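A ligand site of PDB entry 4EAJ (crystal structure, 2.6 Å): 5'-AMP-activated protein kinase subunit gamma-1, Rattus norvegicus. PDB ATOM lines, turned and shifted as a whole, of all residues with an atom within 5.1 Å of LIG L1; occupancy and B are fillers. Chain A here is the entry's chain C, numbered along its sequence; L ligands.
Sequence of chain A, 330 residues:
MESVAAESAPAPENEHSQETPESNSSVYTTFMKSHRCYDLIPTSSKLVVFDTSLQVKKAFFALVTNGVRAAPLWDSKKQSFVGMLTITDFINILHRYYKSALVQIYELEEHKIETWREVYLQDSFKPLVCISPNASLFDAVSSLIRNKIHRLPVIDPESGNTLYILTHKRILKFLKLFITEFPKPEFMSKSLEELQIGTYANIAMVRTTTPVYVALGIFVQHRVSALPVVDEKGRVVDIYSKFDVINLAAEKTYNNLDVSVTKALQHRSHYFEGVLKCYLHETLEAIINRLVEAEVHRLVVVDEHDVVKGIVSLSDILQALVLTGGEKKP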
ATOM      1  N   ARG A  69      -0.171  -6.753 -22.658  1.00  0.00           N
ATOM      2  CA  ARG A  69      -0.033  -8.116 -23.184  1.00  0.00           C
ATOM      3  C   ARG A  69       0.116  -8.193 -24.703  1.00  0.00           C
ATOM      4  O   ARG A  69       0.326  -9.268 -25.264  1.00  0.00           O
ATOM      5  CB  ARG A  69      -1.225  -8.992 -22.749  1.00  0.00           C
ATOM      6  CG  ARG A  69      -1.134  -9.548 -21.340  1.00  0.00           C
ATOM      7  CD  ARG A  69      -1.846 -10.891 -21.239  1.00  0.00           C
ATOM      8  NE  ARG A  69      -1.562 -11.724 -22.403  1.00  0.00           N
ATOM      9  CZ  ARG A  69      -1.682 -13.055 -22.441  1.00  0.00           C
ATOM     10  NH1 ARG A  69      -2.077 -13.737 -21.377  1.00  0.00           N
ATOM     11  NH2 ARG A  69      -1.384 -13.698 -23.564  1.00  0.00           N
ATOM     12  N   ARG A 151      -6.772 -10.703 -29.449  1.00  0.00           N
ATOM     13  CA  ARG A 151      -6.511  -9.269 -29.380  1.00  0.00           C
ATOM     14  C   ARG A 151      -7.089  -8.578 -30.593  1.00  0.00           C
ATOM     15  O   ARG A 151      -6.563  -8.706 -31.692  1.00  0.00           O
ATOM     16  CB  ARG A 151      -5.005  -9.016 -29.325  1.00  0.00           C
ATOM     17  CG  ARG A 151      -4.253  -9.952 -28.376  1.00  0.00           C
ATOM     18  CD  ARG A 151      -4.551  -9.641 -26.917  1.00  0.00           C
ATOM     19  NE  ARG A 151      -4.335 -10.809 -26.083  1.00  0.00           N
ATOM     20  CZ  ARG A 151      -4.397 -10.823 -24.764  1.00  0.00           C
ATOM     21  NH1 ARG A 151      -4.664  -9.707 -24.098  1.00  0.00           N
ATOM     22  NH2 ARG A 151      -4.187 -11.950 -24.100  1.00  0.00           N
ATOM     23  N   THR A 167     -10.855  -7.498 -25.839  1.00  0.00           N
ATOM     24  CA  THR A 167     -10.590  -8.882 -25.436  1.00  0.00           C
ATOM     25  C   THR A 167     -11.862  -9.609 -25.031  1.00  0.00           C
ATOM     26  O   THR A 167     -12.907  -8.998 -24.829  1.00  0.00           O
ATOM     27  CB  THR A 167      -9.586  -8.943 -24.266  1.00  0.00           C
ATOM     28  OG1 THR A 167     -10.116  -8.272 -23.111  1.00  0.00           O
ATOM     29  CG2 THR A 167      -8.250  -8.304 -24.654  1.00  0.00           C
ATOM     30  N   LYS A 169     -12.316 -11.144 -22.238  1.00  0.00           N
ATOM     31  CA  LYS A 169     -12.595 -10.816 -20.851  1.00  0.00           C
ATOM     32  C   LYS A 169     -13.431  -9.557 -20.757  1.00  0.00           C
ATOM     33  O   LYS A 169     -14.455  -9.526 -20.079  1.00  0.00           O
ATOM     34  CB  LYS A 169     -11.278 -10.661 -20.088  1.00  0.00           C
ATOM     35  CG  LYS A 169     -11.401 -10.752 -18.580  1.00  0.00           C
ATOM     36  CD  LYS A 169     -10.039 -10.657 -17.919  1.00  0.00           C
ATOM     37  CE  LYS A 169      -9.172 -11.875 -18.219  1.00  0.00           C
ATOM     38  NZ  LYS A 169      -7.870 -11.810 -17.502  1.00  0.00           N
ATOM     39  N   ILE A 239      -1.784 -23.847 -12.171  1.00  0.00           N
ATOM     40  CA  ILE A 239      -2.023 -23.494 -13.562  1.00  0.00           C
ATOM     41  C   ILE A 239      -0.868 -22.650 -14.100  1.00  0.00           C
ATOM     42  O   ILE A 239      -0.443 -21.660 -13.483  1.00  0.00           O
ATOM     43  CB  ILE A 239      -3.350 -22.713 -13.702  1.00  0.00           C
ATOM     44  CG1 ILE A 239      -3.668 -22.453 -15.170  1.00  0.00           C
ATOM     45  CG2 ILE A 239      -3.309 -21.410 -12.917  1.00  0.00           C
ATOM     46  CD1 ILE A 239      -4.548 -23.506 -15.787  1.00  0.00           C
ATOM     47  N   SER A 241       0.081 -20.320 -17.060  1.00  0.00           N
ATOM     48  CA  SER A 241      -0.473 -19.554 -18.179  1.00  0.00           C
ATOM     49  C   SER A 241       0.625 -19.028 -19.094  1.00  0.00           C
ATOM     50  O   SER A 241       1.806 -19.092 -18.751  1.00  0.00           O
ATOM     51  CB  SER A 241      -1.327 -18.381 -17.655  1.00  0.00           C
ATOM     52  OG  SER A 241      -2.093 -17.770 -18.682  1.00  0.00           O
ATOM     53  N   PHE A 243       0.682 -15.942 -19.856  1.00  0.00           N
ATOM     54  CA  PHE A 243       0.947 -14.702 -19.131  1.00  0.00           C
ATOM     55  C   PHE A 243       2.069 -14.872 -18.116  1.00  0.00           C
ATOM     56  O   PHE A 243       2.789 -13.927 -17.814  1.00  0.00           O
ATOM     57  CB  PHE A 243      -0.343 -14.237 -18.434  1.00  0.00           C
ATOM     58  CG  PHE A 243      -0.126 -13.112 -17.460  1.00  0.00           C
ATOM     59  CD1 PHE A 243       0.287 -11.865 -17.893  1.00  0.00           C
ATOM     60  CD2 PHE A 243      -0.355 -13.306 -16.110  1.00  0.00           C
ATOM     61  CE1 PHE A 243       0.476 -10.832 -16.999  1.00  0.00           C
ATOM     62  CE2 PHE A 243      -0.165 -12.277 -15.206  1.00  0.00           C
ATOM     63  CZ  PHE A 243       0.249 -11.038 -15.655  1.00  0.00           C
ATOM     64  N   ASP A 244       2.207 -16.082 -17.591  1.00  0.00           N
ATOM     65  CA  ASP A 244       3.235 -16.386 -16.594  1.00  0.00           C
ATOM     66  C   ASP A 244       4.612 -16.574 -17.210  1.00  0.00           C
ATOM     67  O   ASP A 244       5.569 -16.917 -16.511  1.00  0.00           O
ATOM     68  CB  ASP A 244       2.867 -17.663 -15.818  1.00  0.00           C
ATOM     69  CG  ASP A 244       1.613 -17.486 -14.979  1.00  0.00           C
ATOM     70  OD1 ASP A 244       1.554 -16.516 -14.190  1.00  0.00           O
ATOM     71  OD2 ASP A 244       0.691 -18.331 -15.102  1.00  0.00           O
ATOM     72  N   ARG A 268       4.994 -15.552  -8.207  1.00  0.00           N
ATOM     73  CA  ARG A 268       3.591 -15.208  -8.366  1.00  0.00           C
ATOM     74  C   ARG A 268       3.336 -13.789  -7.871  1.00  0.00           C
ATOM     75  O   ARG A 268       3.318 -13.524  -6.671  1.00  0.00           O
ATOM     76  CB  ARG A 268       2.714 -16.197  -7.596  1.00  0.00           C
ATOM     77  CG  ARG A 268       1.231 -16.032  -7.853  1.00  0.00           C
ATOM     78  CD  ARG A 268       0.841 -16.520  -9.240  1.00  0.00           C
ATOM     79  NE  ARG A 268       0.762 -17.975  -9.323  1.00  0.00           N
ATOM     80  CZ  ARG A 268       0.131 -18.632 -10.295  1.00  0.00           C
ATOM     81  NH1 ARG A 268      -0.482 -17.955 -11.264  1.00  0.00           N
ATOM     82  NH2 ARG A 268       0.102 -19.949 -10.287  1.00  0.00           N
ATOM     83  N   PHE A 272      -2.839 -15.201  -4.684  1.00  0.00           N
ATOM     84  CA  PHE A 272      -3.278 -16.432  -5.324  1.00  0.00           C
ATOM     85  C   PHE A 272      -4.017 -17.342  -4.342  1.00  0.00           C
ATOM     86  O   PHE A 272      -3.408 -18.036  -3.539  1.00  0.00           O
ATOM     87  CB  PHE A 272      -2.042 -17.153  -5.902  1.00  0.00           C
ATOM     88  CG  PHE A 272      -2.377 -18.305  -6.814  1.00  0.00           C
ATOM     89  CD1 PHE A 272      -2.143 -19.618  -6.417  1.00  0.00           C
ATOM     90  CD2 PHE A 272      -2.914 -18.068  -8.074  1.00  0.00           C
ATOM     91  CE1 PHE A 272      -2.436 -20.672  -7.258  1.00  0.00           C
ATOM     92  CE2 PHE A 272      -3.213 -19.129  -8.918  1.00  0.00           C
ATOM     93  CZ  PHE A 272      -2.975 -20.427  -8.503  1.00  0.00           C
ATOM     94  N   GLY A 274      -5.593 -19.884  -5.172  1.00  0.00           N
ATOM     95  CA  GLY A 274      -5.491 -21.239  -5.680  1.00  0.00           C
ATOM     96  C   GLY A 274      -6.090 -21.347  -7.069  1.00  0.00           C
ATOM     97  O   GLY A 274      -6.341 -20.330  -7.719  1.00  0.00           O
ATOM     98  N   VAL A 275      -6.323 -22.569  -7.528  1.00  0.00           N
ATOM     99  CA  VAL A 275      -6.834 -22.787  -8.867  1.00  0.00           C
ATOM    100  C   VAL A 275      -8.371 -22.697  -8.922  1.00  0.00           C
ATOM    101  O   VAL A 275      -9.077 -23.302  -8.123  1.00  0.00           O
ATOM    102  CB  VAL A 275      -6.341 -24.124  -9.462  1.00  0.00           C
ATOM    103  CG1 VAL A 275      -6.706 -25.282  -8.557  1.00  0.00           C
ATOM    104  CG2 VAL A 275      -6.901 -24.339 -10.865  1.00  0.00           C
ATOM    105  N   LEU A 276      -8.861 -21.930  -9.888  1.00  0.00           N
ATOM    106  CA  LEU A 276     -10.285 -21.730 -10.086  1.00  0.00           C
ATOM    107  C   LEU A 276     -10.867 -22.810 -10.977  1.00  0.00           C
ATOM    108  O   LEU A 276     -10.463 -22.981 -12.122  1.00  0.00           O
ATOM    109  CB  LEU A 276     -10.536 -20.340 -10.679  1.00  0.00           C
ATOM    110  CG  LEU A 276      -9.725 -19.260  -9.964  1.00  0.00           C
ATOM    111  CD1 LEU A 276      -9.897 -17.916 -10.631  1.00  0.00           C
ATOM    112  CD2 LEU A 276     -10.127 -19.207  -8.507  1.00  0.00           C
ATOM    113  N   GLU A 295     -12.005 -13.042 -13.141  1.00  0.00           N
ATOM    114  CA  GLU A 295     -11.206 -12.291 -14.097  1.00  0.00           C
ATOM    115  C   GLU A 295     -10.017 -13.076 -14.660  1.00  0.00           C
ATOM    116  O   GLU A 295      -8.988 -12.494 -15.032  1.00  0.00           O
ATOM    117  CB  GLU A 295     -10.747 -10.957 -13.507  1.00  0.00           C
ATOM    118  CG  GLU A 295     -11.884  -9.980 -13.244  1.00  0.00           C
ATOM    119  CD  GLU A 295     -11.391  -8.574 -12.934  1.00  0.00           C
ATOM    120  OE1 GLU A 295     -12.151  -7.613 -13.171  1.00  0.00           O
ATOM    121  OE2 GLU A 295     -10.235  -8.432 -12.483  1.00  0.00           O
ATOM    122  N   VAL A 296     -10.174 -14.396 -14.746  1.00  0.00           N
ATOM    123  CA  VAL A 296      -9.204 -15.244 -15.438  1.00  0.00           C
ATOM    124  C   VAL A 296      -9.790 -15.719 -16.770  1.00  0.00           C
ATOM    125  O   VAL A 296     -10.988 -15.642 -16.992  1.00  0.00           O
ATOM    126  CB  VAL A 296      -8.763 -16.433 -14.574  1.00  0.00           C
ATOM    127  CG1 VAL A 296      -8.133 -15.922 -13.283  1.00  0.00           C
ATOM    128  CG2 VAL A 296      -9.943 -17.343 -14.271  1.00  0.00           C
ATOM    129  N   HIS A 297      -8.922 -16.219 -17.646  1.00  0.00           N
ATOM    130  CA  HIS A 297      -9.342 -16.560 -19.000  1.00  0.00           C
ATOM    131  C   HIS A 297     -10.105 -17.892 -19.071  1.00  0.00           C
ATOM    132  O   HIS A 297     -10.805 -18.143 -20.053  1.00  0.00           O
ATOM    133  CB  HIS A 297      -8.134 -16.569 -19.940  1.00  0.00           C
ATOM    134  CG  HIS A 297      -8.504 -16.674 -21.390  1.00  0.00           C
ATOM    135  ND1 HIS A 297      -8.860 -15.575 -22.149  1.00  0.00           N
ATOM    136  CD2 HIS A 297      -8.565 -17.744 -22.223  1.00  0.00           C
ATOM    137  CE1 HIS A 297      -9.130 -15.967 -23.393  1.00  0.00           C
ATOM    138  NE2 HIS A 297      -8.960 -17.268 -23.449  1.00  0.00           N
ATOM    139  N   ARG A 298      -9.984 -18.725 -18.044  1.00  0.00           N
ATOM    140  CA  ARG A 298     -10.666 -20.026 -18.059  1.00  0.00           C
ATOM    141  C   ARG A 298     -10.769 -20.664 -16.689  1.00  0.00           C
ATOM    142  O   ARG A 298     -10.067 -20.279 -15.762  1.00  0.00           O
ATOM    143  CB  ARG A 298      -9.954 -21.000 -19.001  1.00  0.00           C
ATOM    144  CG  ARG A 298      -8.952 -21.928 -18.314  1.00  0.00           C
ATOM    145  CD  ARG A 298      -7.687 -21.181 -17.906  1.00  0.00           C
ATOM    146  NE  ARG A 298      -7.080 -20.525 -19.056  1.00  0.00           N
ATOM    147  CZ  ARG A 298      -6.354 -19.418 -18.998  1.00  0.00           C
ATOM    148  NH1 ARG A 298      -6.122 -18.824 -17.826  1.00  0.00           N
ATOM    149  NH2 ARG A 298      -5.856 -18.893 -20.117  1.00  0.00           N
ATOM    150  N   LEU A 299     -11.673 -21.636 -16.597  1.00  0.00           N
ATOM    151  CA  LEU A 299     -11.794 -22.526 -15.457  1.00  0.00           C
ATOM    152  C   LEU A 299     -11.370 -23.940 -15.850  1.00  0.00           C
ATOM    153  O   LEU A 299     -11.652 -24.398 -16.958  1.00  0.00           O
ATOM    154  CB  LEU A 299     -13.239 -22.593 -14.946  1.00  0.00           C
ATOM    155  CG  LEU A 299     -14.053 -21.342 -14.632  1.00  0.00           C
ATOM    156  CD1 LEU A 299     -15.352 -21.759 -13.951  1.00  0.00           C
ATOM    157  CD2 LEU A 299     -13.266 -20.390 -13.745  1.00  0.00           C
ATOM    158  N   VAL A 300     -10.714 -24.618 -14.928  1.00  0.00           N
ATOM    159  CA  VAL A 300     -10.426 -26.034 -15.097  1.00  0.00           C
ATOM    160  C   VAL A 300     -11.636 -26.843 -14.626  1.00  0.00           C
ATOM    161  O   VAL A 300     -12.018 -26.772 -13.455  1.00  0.00           O
ATOM    162  CB  VAL A 300      -9.208 -26.455 -14.253  1.00  0.00           C
ATOM    163  CG1 VAL A 300      -8.850 -27.905 -14.536  1.00  0.00           C
ATOM    164  CG2 VAL A 300      -8.030 -25.533 -14.550  1.00  0.00           C
ATOM    165  N   LEU A 314     -13.185 -18.563 -21.800  1.00  0.00           N
ATOM    166  CA  LEU A 314     -13.989 -17.445 -22.301  1.00  0.00           C
ATOM    167  C   LEU A 314     -14.335 -17.609 -23.784  1.00  0.00           C
ATOM    168  O   LEU A 314     -15.395 -17.163 -24.219  1.00  0.00           O
ATOM    169  CB  LEU A 314     -13.255 -16.122 -22.098  1.00  0.00           C
ATOM    170  CG  LEU A 314     -12.970 -15.690 -20.665  1.00  0.00           C
ATOM    171  CD1 LEU A 314     -12.215 -14.359 -20.639  1.00  0.00           C
ATOM    172  CD2 LEU A 314     -14.282 -15.605 -19.914  1.00  0.00           C
HETATM  173  P1  LIG L   1      -6.665 -12.222 -21.022  1.00  0.00           P
HETATM  174  O1  LIG L   1      -7.097 -11.001 -21.790  1.00  0.00           O
HETATM  175  O2  LIG L   1      -5.607 -13.046 -21.686  1.00  0.00           O
HETATM  176  O3  LIG L   1      -7.817 -13.040 -20.515  1.00  0.00           O
HETATM  177  P2  LIG L   1      -4.731 -12.408 -18.946  1.00  0.00           P
HETATM  178  O4  LIG L   1      -3.940 -11.336 -18.268  1.00  0.00           O
HETATM  179  O5  LIG L   1      -4.034 -13.288 -19.917  1.00  0.00           O
HETATM  180  O6  LIG L   1      -5.962 -11.673 -19.671  1.00  0.00           O
HETATM  181  P3  LIG L   1      -5.093 -14.918 -17.716  1.00  0.00           P
HETATM  182  O7  LIG L   1      -6.376 -15.615 -17.385  1.00  0.00           O
HETATM  183  O8  LIG L   1      -4.334 -15.351 -18.933  1.00  0.00           O
HETATM  184  O9  LIG L   1      -5.376 -13.334 -17.799  1.00  0.00           O
HETATM  185  O10 LIG L   1      -4.080 -15.086 -16.477  1.00  0.00           O
HETATM  186  C1  LIG L   1      -4.157 -14.198 -15.356  1.00  0.00           C
HETATM  187  C2  LIG L   1      -3.444 -14.837 -14.171  1.00  0.00           C
HETATM  188  O11 LIG L   1      -4.392 -15.592 -13.420  1.00  0.00           O
HETATM  189  C3  LIG L   1      -2.360 -15.785 -14.641  1.00  0.00           C
HETATM  190  O12 LIG L   1      -1.119 -15.453 -14.006  1.00  0.00           O
HETATM  191  C4  LIG L   1      -2.825 -17.160 -14.225  1.00  0.00           C
HETATM  192  O13 LIG L   1      -1.777 -17.914 -13.609  1.00  0.00           O
HETATM  193  C5  LIG L   1      -3.979 -16.945 -13.261  1.00  0.00           C
HETATM  194  N1  LIG L   1      -5.068 -17.859 -13.655  1.00  0.00           N
HETATM  195  C6  LIG L   1      -5.599 -17.946 -14.880  1.00  0.00           C
HETATM  196  N2  LIG L   1      -6.572 -18.882 -14.922  1.00  0.00           N
HETATM  197  C7  LIG L   1      -6.675 -19.427 -13.695  1.00  0.00           C
HETATM  198  C8  LIG L   1      -7.497 -20.484 -13.054  1.00  0.00           C
HETATM  199  N3  LIG L   1      -8.443 -21.157 -13.752  1.00  0.00           N
HETATM  200  N4  LIG L   1      -7.272 -20.745 -11.750  1.00  0.00           N
HETATM  201  C9  LIG L   1      -6.347 -20.078 -11.031  1.00  0.00           C
HETATM  202  N5  LIG L   1      -5.567 -19.123 -11.553  1.00  0.00           N
HETATM  203  C10 LIG L   1      -5.673 -18.755 -12.856  1.00  0.00           C
HETATM  204  P1  LG2 L   2      -3.316 -15.843 -25.280  1.00  0.00           P
HETATM  205  O1  LG2 L   2      -4.470 -14.883 -25.341  1.00  0.00           O
HETATM  206  O2  LG2 L   2      -2.550 -15.800 -23.993  1.00  0.00           O
HETATM  207  O3  LG2 L   2      -3.696 -17.236 -25.704  1.00  0.00           O
HETATM  208  P2  LG2 L   2      -2.279 -13.901 -27.070  1.00  0.00           P
HETATM  209  O4  LG2 L   2      -3.603 -13.244 -26.914  1.00  0.00           O
HETATM  210  O5  LG2 L   2      -1.091 -13.168 -26.551  1.00  0.00           O
HETATM  211  O6  LG2 L   2      -2.301 -15.374 -26.432  1.00  0.00           O
HETATM  212  P3  LG2 L   2      -3.202 -14.417 -29.719  1.00  0.00           P
HETATM  213  O7  LG2 L   2      -4.080 -13.202 -29.815  1.00  0.00           O
HETATM  214  O8  LG2 L   2      -3.799 -15.765 -29.483  1.00  0.00           O
HETATM  215  O9  LG2 L   2      -2.039 -14.200 -28.631  1.00  0.00           O
HETATM  216  O10 LG2 L   2      -2.311 -14.438 -31.049  1.00  0.00           O
HETATM  217  C1  LG2 L   2      -1.993 -15.613 -31.772  1.00  0.00           C
HETATM  218  C2  LG2 L   2      -1.209 -15.129 -32.990  1.00  0.00           C
HETATM  219  O11 LG2 L   2      -2.078 -14.279 -33.749  1.00  0.00           O
HETATM  220  C3  LG2 L   2      -0.021 -14.297 -32.566  1.00  0.00           C
HETATM  221  O12 LG2 L   2       1.117 -14.704 -33.324  1.00  0.00           O
HETATM  222  C4  LG2 L   2      -0.387 -12.868 -32.916  1.00  0.00           C
HETATM  223  O13 LG2 L   2       0.720 -12.176 -33.485  1.00  0.00           O
HETATM  224  C5  LG2 L   2      -1.515 -12.986 -33.921  1.00  0.00           C
HETATM  225  N1  LG2 L   2      -2.536 -11.930 -33.682  1.00  0.00           N
HETATM  226  C6  LG2 L   2      -3.083 -11.617 -32.498  1.00  0.00           C
HETATM  227  N2  LG2 L   2      -3.966 -10.602 -32.629  1.00  0.00           N
HETATM  228  C7  LG2 L   2      -4.007 -10.240 -33.917  1.00  0.00           C
HETATM  229  C8  LG2 L   2      -4.728  -9.236 -34.743  1.00  0.00           C
HETATM  230  N3  LG2 L   2      -5.625  -8.388 -34.181  1.00  0.00           N
HETATM  231  N4  LG2 L   2      -4.445  -9.212 -36.061  1.00  0.00           N
HETATM  232  C9  LG2 L   2      -3.565 -10.040 -36.634  1.00  0.00           C
HETATM  233  N5  LG2 L   2      -2.877 -10.968 -35.947  1.00  0.00           N
HETATM  234  C10 LG2 L   2      -3.047 -11.120 -34.613  1.00  0.00           C
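The guanidinium group (NH1) of Arg 69 is in salt-bridge range of an oxygen (O5) of LIG L1 (2.5 Å).
O7 of LIG L1 lies within hydrogen-bond range of N of His 297 (2.6 Å).
An oxygen (O3) of LIG L1 sits at hydrogen-bond distance from a ring nitrogen (ND1) of His 297 (3.2 Å).
O13 of LIG L1 sits at hydrogen-bond distance from NH1 of Arg 268, 2.7 Å away.
N of Leu 276 sits at hydrogen-bond distance from N4 of LIG L1, 2.7 Å away.
O of Leu 276 lies within hydrogen-bond range of N3 of LIG L1 (3.2 Å).
A nitrogen (N3) of LIG L1 lies within hydrogen-bond range of the backbone carbonyl oxygen of Arg 298.
The guanidinium group of Arg 298 is in salt-bridge range of an oxygen (O7) of LIG L1 (3.2 Å).
The side-chain carboxylate of Asp 244 lies within hydrogen-bond range of an oxygen (O12) of LIG L1.
The side-chain amino group of Lys 169 is in salt-bridge range of an oxygen (O3) of LIG L1 (3.3 Å).
The guanidinium group of Arg 151 is in salt-bridge range of an oxygen (O2) of LIG L1.
The side-chain hydroxyl (OG) of Ser 241 lies within hydrogen-bond range of an oxygen (O8) of LIG L1.
An oxygen (O2) of LG2 L2 lies within salt-bridge range of the guanidinium group of Arg 69, 2.4 Å away.
O of Arg 151 sits at hydrogen-bond distance from N3 of LG2 L2 (2.7 Å).
The guanidinium group (NE) of Arg 151 is in salt-bridge range of an oxygen (O4) of LG2 L2 (2.7 Å).
The backbone carbonyl oxygen (O) of His 297 is in hydrogen-bond range of the backbone NH (N) of Leu 314 (3.0 Å).
The side-chain carboxylate (OD1) of Asp 244 is in salt-bridge range of the guanidinium group (NH1) of Arg 268.
The backbone carbonyl oxygen (O) of Leu 276 lies within hydrogen-bond range of the backbone NH (N) of Val 300 (3.3 Å).
The backbone NH (N) of Ser 241 is in hydrogen-bond range of the side-chain carboxylate (OD2) of Asp 244 (2.9 Å).
The backbone carbonyl oxygen (O) of Glu 295 sits at hydrogen-bond distance from the side-chain amino group (NZ) of Lys 169, at 2.8 Å.
Residues that only touch LIG L1: Phe 243 (3.1 Å), Val 296 (3.3 Å), Gly 274 (3.3 Å), Ile 239 (3.5 Å), Val 275 (3.5 Å) and Phe 272 (3.5 Å).
15 residues have an atom within 4 Å of LIG L1: Arg 69, Arg 151, Lys 169, Ile 239, Ser 241, Phe 243, Asp 244, Arg 268, Phe 272, Gly 274, Val 275, Leu 276, Val 296, His 297 and Arg 298.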
